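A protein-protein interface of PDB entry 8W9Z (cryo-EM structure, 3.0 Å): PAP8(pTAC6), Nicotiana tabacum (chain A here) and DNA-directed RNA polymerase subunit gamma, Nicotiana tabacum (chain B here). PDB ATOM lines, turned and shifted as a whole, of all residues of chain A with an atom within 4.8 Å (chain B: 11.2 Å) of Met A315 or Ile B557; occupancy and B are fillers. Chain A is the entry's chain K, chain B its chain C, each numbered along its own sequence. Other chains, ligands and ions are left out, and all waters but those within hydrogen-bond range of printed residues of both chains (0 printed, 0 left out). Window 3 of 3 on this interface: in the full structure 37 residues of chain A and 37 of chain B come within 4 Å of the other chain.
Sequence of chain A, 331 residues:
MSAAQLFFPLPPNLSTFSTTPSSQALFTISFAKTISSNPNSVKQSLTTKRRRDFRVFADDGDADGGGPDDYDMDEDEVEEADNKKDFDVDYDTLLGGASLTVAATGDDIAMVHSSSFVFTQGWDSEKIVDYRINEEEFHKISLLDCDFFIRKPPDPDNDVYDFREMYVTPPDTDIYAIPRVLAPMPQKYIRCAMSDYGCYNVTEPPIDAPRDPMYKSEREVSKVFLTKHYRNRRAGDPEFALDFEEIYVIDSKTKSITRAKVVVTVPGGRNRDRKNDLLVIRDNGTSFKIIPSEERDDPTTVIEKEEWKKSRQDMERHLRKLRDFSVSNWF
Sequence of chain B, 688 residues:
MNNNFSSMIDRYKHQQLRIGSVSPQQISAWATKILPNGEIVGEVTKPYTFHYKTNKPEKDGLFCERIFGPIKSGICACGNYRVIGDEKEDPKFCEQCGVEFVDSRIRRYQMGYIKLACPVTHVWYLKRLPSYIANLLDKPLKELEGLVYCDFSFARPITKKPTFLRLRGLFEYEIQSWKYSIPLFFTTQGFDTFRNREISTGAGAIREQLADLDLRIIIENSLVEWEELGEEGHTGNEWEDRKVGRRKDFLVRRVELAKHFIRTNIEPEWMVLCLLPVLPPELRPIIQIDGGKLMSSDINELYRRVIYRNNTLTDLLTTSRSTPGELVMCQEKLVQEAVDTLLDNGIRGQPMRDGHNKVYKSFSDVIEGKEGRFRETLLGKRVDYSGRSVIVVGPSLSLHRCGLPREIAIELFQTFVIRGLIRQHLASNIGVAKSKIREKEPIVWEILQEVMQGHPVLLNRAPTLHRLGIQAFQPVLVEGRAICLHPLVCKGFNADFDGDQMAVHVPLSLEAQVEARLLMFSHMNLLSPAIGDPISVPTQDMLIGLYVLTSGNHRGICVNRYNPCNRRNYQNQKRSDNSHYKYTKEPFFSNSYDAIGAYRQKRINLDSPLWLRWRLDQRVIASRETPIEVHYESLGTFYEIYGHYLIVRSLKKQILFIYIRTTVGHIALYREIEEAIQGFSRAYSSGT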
ATOM      1  N   TRP A 308      23.477   3.527  10.002  1.00  0.00           N
ATOM      2  CA  TRP A 308      22.803   2.571  10.871  1.00  0.00           C
ATOM      3  C   TRP A 308      23.544   2.414  12.190  1.00  0.00           C
ATOM      4  O   TRP A 308      22.920   2.385  13.258  1.00  0.00           O
ATOM      5  CB  TRP A 308      22.684   1.226  10.155  1.00  0.00           C
ATOM      6  CG  TRP A 308      21.686   0.288  10.758  1.00  0.00           C
ATOM      7  CD1 TRP A 308      20.365   0.186  10.438  1.00  0.00           C
ATOM      8  CD2 TRP A 308      21.931  -0.691  11.772  1.00  0.00           C
ATOM      9  NE1 TRP A 308      19.769  -0.793  11.195  1.00  0.00           N
ATOM     10  CE2 TRP A 308      20.710  -1.347  12.022  1.00  0.00           C
ATOM     11  CE3 TRP A 308      23.063  -1.076  12.496  1.00  0.00           C
ATOM     12  CZ2 TRP A 308      20.589  -2.363  12.965  1.00  0.00           C
ATOM     13  CZ3 TRP A 308      22.940  -2.085  13.430  1.00  0.00           C
ATOM     14  CH2 TRP A 308      21.713  -2.717  13.656  1.00  0.00           C
ATOM     15  N   SER A 311      23.031   5.615  14.255  1.00  0.00           N
ATOM     16  CA  SER A 311      21.654   5.726  14.720  1.00  0.00           C
ATOM     17  C   SER A 311      21.367   4.737  15.838  1.00  0.00           C
ATOM     18  O   SER A 311      20.663   5.068  16.797  1.00  0.00           O
ATOM     19  CB  SER A 311      20.690   5.514  13.554  1.00  0.00           C
ATOM     20  OG  SER A 311      20.867   4.234  12.976  1.00  0.00           O
ATOM     21  N   ARG A 312      21.910   3.521  15.744  1.00  0.00           N
ATOM     22  CA  ARG A 312      21.702   2.551  16.812  1.00  0.00           C
ATOM     23  C   ARG A 312      22.396   2.987  18.094  1.00  0.00           C
ATOM     24  O   ARG A 312      21.838   2.841  19.189  1.00  0.00           O
ATOM     25  CB  ARG A 312      22.193   1.172  16.381  1.00  0.00           C
ATOM     26  CG  ARG A 312      21.988   0.106  17.435  1.00  0.00           C
ATOM     27  CD  ARG A 312      22.349  -1.260  16.905  1.00  0.00           C
ATOM     28  NE  ARG A 312      22.149  -2.301  17.908  1.00  0.00           N
ATOM     29  CZ  ARG A 312      22.307  -3.597  17.671  1.00  0.00           C
ATOM     30  NH1 ARG A 312      22.665  -4.014  16.465  1.00  0.00           N
ATOM     31  NH2 ARG A 312      22.108  -4.478  18.639  1.00  0.00           N
ATOM     32  N   GLN A 313      23.613   3.528  17.980  1.00  0.00           N
ATOM     33  CA  GLN A 313      24.292   4.035  19.169  1.00  0.00           C
ATOM     34  C   GLN A 313      23.491   5.156  19.820  1.00  0.00           C
ATOM     35  O   GLN A 313      23.315   5.173  21.046  1.00  0.00           O
ATOM     36  CB  GLN A 313      25.699   4.513  18.811  1.00  0.00           C
ATOM     37  CG  GLN A 313      26.638   3.403  18.365  1.00  0.00           C
ATOM     38  CD  GLN A 313      26.940   2.410  19.471  1.00  0.00           C
ATOM     39  OE1 GLN A 313      27.148   1.224  19.215  1.00  0.00           O
ATOM     40  NE2 GLN A 313      26.975   2.892  20.708  1.00  0.00           N
ATOM     41  N   ASP A 314      22.980   6.090  19.014  1.00  0.00           N
ATOM     42  CA  ASP A 314      22.192   7.190  19.564  1.00  0.00           C
ATOM     43  C   ASP A 314      20.898   6.689  20.196  1.00  0.00           C
ATOM     44  O   ASP A 314      20.483   7.187  21.249  1.00  0.00           O
ATOM     45  CB  ASP A 314      21.894   8.218  18.473  1.00  0.00           C
ATOM     46  CG  ASP A 314      23.150   8.852  17.911  1.00  0.00           C
ATOM     47  OD1 ASP A 314      24.143   8.971  18.659  1.00  0.00           O
ATOM     48  OD2 ASP A 314      23.146   9.229  16.721  1.00  0.00           O
ATOM     49  N   MET A 315      20.252   5.698  19.577  1.00  0.00           N
ATOM     50  CA  MET A 315      19.005   5.173  20.123  1.00  0.00           C
ATOM     51  C   MET A 315      19.236   4.470  21.453  1.00  0.00           C
ATOM     52  O   MET A 315      18.450   4.638  22.394  1.00  0.00           O
ATOM     53  CB  MET A 315      18.353   4.221  19.123  1.00  0.00           C
ATOM     54  CG  MET A 315      16.933   3.823  19.482  1.00  0.00           C
ATOM     55  SD  MET A 315      15.801   5.225  19.435  1.00  0.00           S
ATOM     56  CE  MET A 315      14.264   4.444  19.911  1.00  0.00           C
ATOM     57  N   GLU A 316      20.306   3.678  21.553  1.00  0.00           N
ATOM     58  CA  GLU A 316      20.615   3.031  22.824  1.00  0.00           C
ATOM     59  C   GLU A 316      20.973   4.058  23.890  1.00  0.00           C
ATOM     60  O   GLU A 316      20.565   3.924  25.051  1.00  0.00           O
ATOM     61  CB  GLU A 316      21.744   2.020  22.641  1.00  0.00           C
ATOM     62  CG  GLU A 316      21.380   0.853  21.736  1.00  0.00           C
ATOM     63  CD  GLU A 316      22.515  -0.135  21.565  1.00  0.00           C
ATOM     64  OE1 GLU A 316      23.570   0.050  22.208  1.00  0.00           O
ATOM     65  OE2 GLU A 316      22.354  -1.098  20.786  1.00  0.00           O
ATOM     66  N   ARG A 317      21.548   5.175  23.514  1.00  0.00           N
ATOM     67  CA  ARG A 317      21.818   6.204  24.508  1.00  0.00           C
ATOM     68  C   ARG A 317      20.546   6.804  25.036  1.00  0.00           C
ATOM     69  O   ARG A 317      20.404   7.003  26.225  1.00  0.00           O
ATOM     70  CB  ARG A 317      22.656   7.307  23.914  1.00  0.00           C
ATOM     71  CG  ARG A 317      23.329   8.204  24.925  1.00  0.00           C
ATOM     72  CD  ARG A 317      23.980   9.385  24.228  1.00  0.00           C
ATOM     73  NE  ARG A 317      24.463   9.047  22.891  1.00  0.00           N
ATOM     74  CZ  ARG A 317      25.664   8.542  22.629  1.00  0.00           C
ATOM     75  NH1 ARG A 317      26.515   8.299  23.615  1.00  0.00           N
ATOM     76  NH2 ARG A 317      26.013   8.273  21.379  1.00  0.00           N
ATOM     77  N   HIS A 318      19.617   7.122  24.156  1.00  0.00           N
ATOM     78  CA  HIS A 318      18.384   7.761  24.580  1.00  0.00           C
ATOM     79  C   HIS A 318      17.600   6.869  25.472  1.00  0.00           C
ATOM     80  O   HIS A 318      17.040   7.316  26.435  1.00  0.00           O
ATOM     81  CB  HIS A 318      17.536   8.121  23.379  1.00  0.00           C
ATOM     82  CG  HIS A 318      16.204   8.706  23.711  1.00  0.00           C
ATOM     83  ND1 HIS A 318      16.053   9.988  24.189  1.00  0.00           N
ATOM     84  CD2 HIS A 318      14.955   8.200  23.589  1.00  0.00           C
ATOM     85  CE1 HIS A 318      14.770  10.237  24.374  1.00  0.00           C
ATOM     86  NE2 HIS A 318      14.081   9.169  24.015  1.00  0.00           N
ATOM     87  N   LEU A 319      17.537   5.597  25.159  1.00  0.00           N
ATOM     88  CA  LEU A 319      16.716   4.716  25.940  1.00  0.00           C
ATOM     89  C   LEU A 319      17.407   4.300  27.226  1.00  0.00           C
ATOM     90  O   LEU A 319      16.740   3.916  28.165  1.00  0.00           O
ATOM     91  CB  LEU A 319      16.294   3.503  25.133  1.00  0.00           C
ATOM     92  CG  LEU A 319      15.460   3.740  23.884  1.00  0.00           C
ATOM     93  CD1 LEU A 319      15.167   2.407  23.225  1.00  0.00           C
ATOM     94  CD2 LEU A 319      14.169   4.445  24.245  1.00  0.00           C
ATOM     95  N   TRP A 330      15.577  -5.511  22.128  1.00  0.00           N
ATOM     96  CA  TRP A 330      15.761  -4.659  20.957  1.00  0.00           C
ATOM     97  C   TRP A 330      15.306  -5.439  19.729  1.00  0.00           C
ATOM     98  O   TRP A 330      16.053  -6.258  19.189  1.00  0.00           O
ATOM     99  CB  TRP A 330      17.213  -4.209  20.824  1.00  0.00           C
ATOM    100  CG  TRP A 330      17.398  -3.079  19.856  1.00  0.00           C
ATOM    101  CD1 TRP A 330      17.311  -1.744  20.128  1.00  0.00           C
ATOM    102  CD2 TRP A 330      17.699  -3.183  18.459  1.00  0.00           C
ATOM    103  NE1 TRP A 330      17.541  -1.012  18.989  1.00  0.00           N
ATOM    104  CE2 TRP A 330      17.781  -1.873  17.951  1.00  0.00           C
ATOM    105  CE3 TRP A 330      17.909  -4.257  17.591  1.00  0.00           C
ATOM    106  CZ2 TRP A 330      18.064  -1.608  16.615  1.00  0.00           C
ATOM    107  CZ3 TRP A 330      18.189  -3.992  16.265  1.00  0.00           C
ATOM    108  CH2 TRP A 330      18.265  -2.678  15.790  1.00  0.00           C
ATOM    109  N   ASN B 553      13.987  12.321   5.219  1.00  0.00           N
ATOM    110  CA  ASN B 553      13.344  11.136   5.776  1.00  0.00           C
ATOM    111  C   ASN B 553      14.324  10.471   6.736  1.00  0.00           C
ATOM    112  O   ASN B 553      15.386  11.020   7.046  1.00  0.00           O
ATOM    113  CB  ASN B 553      12.891  10.188   4.660  1.00  0.00           C
ATOM    114  CG  ASN B 553      11.822   9.212   5.119  1.00  0.00           C
ATOM    115  OD1 ASN B 553      12.116   8.065   5.454  1.00  0.00           O
ATOM    116  ND2 ASN B 553      10.576   9.667   5.143  1.00  0.00           N
ATOM    117  N   HIS B 554      13.961   9.283   7.212  1.00  0.00           N
ATOM    118  CA  HIS B 554      14.824   8.536   8.113  1.00  0.00           C
ATOM    119  C   HIS B 554      16.078   8.071   7.383  1.00  0.00           C
ATOM    120  O   HIS B 554      16.092   7.912   6.160  1.00  0.00           O
ATOM    121  CB  HIS B 554      14.070   7.338   8.687  1.00  0.00           C
ATOM    122  CG  HIS B 554      12.690   7.668   9.167  1.00  0.00           C
ATOM    123  ND1 HIS B 554      11.602   7.726   8.321  1.00  0.00           N
ATOM    124  CD2 HIS B 554      12.223   7.967  10.402  1.00  0.00           C
ATOM    125  CE1 HIS B 554      10.524   8.041   9.016  1.00  0.00           C
ATOM    126  NE2 HIS B 554      10.873   8.192  10.281  1.00  0.00           N
ATOM    127  N   ARG B 555      17.146   7.850   8.150  1.00  0.00           N
ATOM    128  CA  ARG B 555      18.439   7.501   7.578  1.00  0.00           C
ATOM    129  C   ARG B 555      19.099   6.276   8.194  1.00  0.00           C
ATOM    130  O   ARG B 555      19.950   5.669   7.534  1.00  0.00           O
ATOM    131  CB  ARG B 555      19.413   8.684   7.692  1.00  0.00           C
ATOM    132  CG  ARG B 555      18.926   9.962   7.029  1.00  0.00           C
ATOM    133  CD  ARG B 555      19.911  11.101   7.237  1.00  0.00           C
ATOM    134  NE  ARG B 555      19.424  12.356   6.673  1.00  0.00           N
ATOM    135  CZ  ARG B 555      18.686  13.237   7.340  1.00  0.00           C
ATOM    136  NH1 ARG B 555      18.287  14.355   6.747  1.00  0.00           N
ATOM    137  NH2 ARG B 555      18.345  13.003   8.599  1.00  0.00           N
ATOM    138  N   GLY B 556      18.748   5.890   9.418  1.00  0.00           N
ATOM    139  CA  GLY B 556      19.446   4.806  10.080  1.00  0.00           C
ATOM    140  C   GLY B 556      18.594   3.591  10.382  1.00  0.00           C
ATOM    141  O   GLY B 556      18.127   2.906   9.469  1.00  0.00           O
ATOM    142  N   ILE B 557      18.390   3.311  11.672  1.00  0.00           N
ATOM    143  CA  ILE B 557      17.623   2.140  12.075  1.00  0.00           C
ATOM    144  C   ILE B 557      16.156   2.257  11.690  1.00  0.00           C
ATOM    145  O   ILE B 557      15.437   1.251  11.687  1.00  0.00           O
ATOM    146  CB  ILE B 557      17.755   1.904  13.590  1.00  0.00           C
ATOM    147  CG1 ILE B 557      17.271   3.132  14.364  1.00  0.00           C
ATOM    148  CG2 ILE B 557      19.192   1.572  13.956  1.00  0.00           C
ATOM    149  CD1 ILE B 557      17.307   2.958  15.861  1.00  0.00           C
ATOM    150  N   CYS B 558      15.687   3.462  11.364  1.00  0.00           N
ATOM    151  CA  CYS B 558      14.283   3.658  11.032  1.00  0.00           C
ATOM    152  C   CYS B 558      13.972   3.357   9.573  1.00  0.00           C
ATOM    153  O   CYS B 558      12.793   3.265   9.214  1.00  0.00           O
ATOM    154  CB  CYS B 558      13.863   5.090  11.367  1.00  0.00           C
ATOM    155  SG  CYS B 558      14.145   5.573  13.085  1.00  0.00           S
ATOM    156  N   VAL B 559      14.989   3.204   8.725  1.00  0.00           N
ATOM    157  CA  VAL B 559      14.776   2.874   7.326  1.00  0.00           C
ATOM    158  C   VAL B 559      15.198   1.445   6.993  1.00  0.00           C
ATOM    159  O   VAL B 559      14.628   0.843   6.077  1.00  0.00           O
ATOM    160  CB  VAL B 559      15.495   3.888   6.408  1.00  0.00           C
ATOM    161  CG1 VAL B 559      17.005   3.759   6.533  1.00  0.00           C
ATOM    162  CG2 VAL B 559      15.047   3.725   4.962  1.00  0.00           C
ATOM    163  N   ASN B 560      16.163   0.880   7.715  1.00  0.00           N
ATOM    164  CA  ASN B 560      16.578  -0.504   7.542  1.00  0.00           C
ATOM    165  C   ASN B 560      16.391  -1.255   8.852  1.00  0.00           C
ATOM    166  O   ASN B 560      16.668  -0.717   9.929  1.00  0.00           O
ATOM    167  CB  ASN B 560      18.041  -0.602   7.094  1.00  0.00           C
ATOM    168  CG  ASN B 560      18.227  -0.264   5.630  1.00  0.00           C
ATOM    169  OD1 ASN B 560      18.124  -1.132   4.764  1.00  0.00           O
ATOM    170  ND2 ASN B 560      18.511   1.000   5.345  1.00  0.00           N
ATOM    171  N   ARG B 561      15.925  -2.499   8.758  1.00  0.00           N
ATOM    172  CA  ARG B 561      15.698  -3.292   9.960  1.00  0.00           C
ATOM    173  C   ARG B 561      16.994  -3.913  10.467  1.00  0.00           C
ATOM    174  O   ARG B 561      17.373  -3.727  11.627  1.00  0.00           O
ATOM    175  CB  ARG B 561      14.654  -4.379   9.693  1.00  0.00           C
ATOM    176  CG  ARG B 561      14.324  -5.206  10.923  1.00  0.00           C
ATOM    177  CD  ARG B 561      13.341  -6.320  10.616  1.00  0.00           C
ATOM    178  NE  ARG B 561      13.052  -7.121  11.801  1.00  0.00           N
ATOM    179  CZ  ARG B 561      12.238  -8.172  11.812  1.00  0.00           C
ATOM    180  NH1 ARG B 561      12.033  -8.842  12.937  1.00  0.00           N
ATOM    181  NH2 ARG B 561      11.628  -8.552  10.698  1.00  0.00           N
ATOM    182  N   TYR B 562      17.684  -4.654   9.609  1.00  0.00           N
ATOM    183  CA  TYR B 562      18.929  -5.313   9.968  1.00  0.00           C
ATOM    184  C   TYR B 562      20.124  -4.499   9.484  1.00  0.00           C
ATOM    185  O   TYR B 562      19.997  -3.566   8.689  1.00  0.00           O
ATOM    186  CB  TYR B 562      18.970  -6.730   9.388  1.00  0.00           C
ATOM    187  CG  TYR B 562      17.907  -7.647   9.947  1.00  0.00           C
ATOM    188  CD1 TYR B 562      17.431  -7.481  11.240  1.00  0.00           C
ATOM    189  CD2 TYR B 562      17.378  -8.676   9.183  1.00  0.00           C
ATOM    190  CE1 TYR B 562      16.461  -8.316  11.756  1.00  0.00           C
ATOM    191  CE2 TYR B 562      16.407  -9.515   9.690  1.00  0.00           C
ATOM    192  CZ  TYR B 562      15.952  -9.330  10.976  1.00  0.00           C
ATOM    193  OH  TYR B 562      14.984 -10.165  11.486  1.00  0.00           O
ATOM    194  N   ASN B 563      21.297  -4.865   9.985  1.00  0.00           N
ATOM    195  CA  ASN B 563      22.514  -4.138   9.649  1.00  0.00           C
ATOM    196  C   ASN B 563      22.847  -4.335   8.174  1.00  0.00           C
ATOM    197  O   ASN B 563      22.922  -5.478   7.707  1.00  0.00           O
ATOM    198  CB  ASN B 563      23.671  -4.614  10.526  1.00  0.00           C
ATOM    199  CG  ASN B 563      24.840  -3.646  10.534  1.00  0.00           C
ATOM    200  OD1 ASN B 563      25.210  -3.088   9.502  1.00  0.00           O
ATOM    201  ND2 ASN B 563      25.428  -3.444  11.706  1.00  0.00           N
ATOM    202  N   PRO B 564      23.049  -3.258   7.409  1.00  0.00           N
ATOM    203  CA  PRO B 564      23.369  -3.404   5.981  1.00  0.00           C
ATOM    204  C   PRO B 564      24.727  -4.030   5.702  1.00  0.00           C
ATOM    205  O   PRO B 564      25.117  -4.117   4.532  1.00  0.00           O
ATOM    206  CB  PRO B 564      23.319  -1.959   5.462  1.00  0.00           C
ATOM    207  CG  PRO B 564      22.511  -1.212   6.470  1.00  0.00           C
ATOM    208  CD  PRO B 564      22.825  -1.852   7.782  1.00  0.00           C
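N of Ile B557 is in hydrogen-bond range of OG of Ser A311 (2.9 Å). The indole nitrogen (NE1) of Trp A308 lies within hydrogen-bond range of the backbone carbonyl oxygen (O) of Asn B560.
The backbone carbonyl oxygen (O) of Trp A308 lies within hydrogen-bond range of the side-chain hydroxyl (OG) of Ser A311, at 2.8 Å. NE of Arg A312 lies within salt-bridge range of OE2 of Glu A316 (3.1 Å).
Of chain B, only Ile B557 comes within 4 Å of Met A315. Of chain A, only Trp A308 (3.7 Å), Ser A311 (2.9 Å), Arg A312 (3.8 Å) and Met A315 (3.7 Å) come within 4 Å of Ile B557. Of the printed residues of chain B, Trp A308 touches Gly B556 (3.7 Å), Ile B557 (3.7 Å), Asn B560 (3.4 Å), Arg B561 (3.7 Å), Tyr B562 (3.7 Å), Asn B563 (3.3 Å) and Pro B564 (3.8 Å). Of chain B, only Gly B556 and Ile B557 come within 4 Å of Ser A311. No residue of chain B comes within 4 Å of Asp A314. Of the printed residues of chain A, Arg B561 touches Trp A308. Of the printed residues of chain A, Gly B556 touches Trp A308 and Ser A311. Arg B555 touches none of the printed residues of chain A.
Gly B556 touches Trp A308. Trp A308 touches Ile B557. Trp A308 touches Arg B561 (CZ2 to O, 3.7 Å). Trp A308 touches Tyr B562 (NE1 to O, 3.7 Å). ND2 of Asn B563 touches CZ3 of Trp A308 (3.3 Å). Trp A308 touches Pro B564 (CG to CD, 3.8 Å). Ser A311 touches Gly B556. Arg A312 touches Ile B557 (N to CG2, 3.8 Å). Ile B557 touches Met A315.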
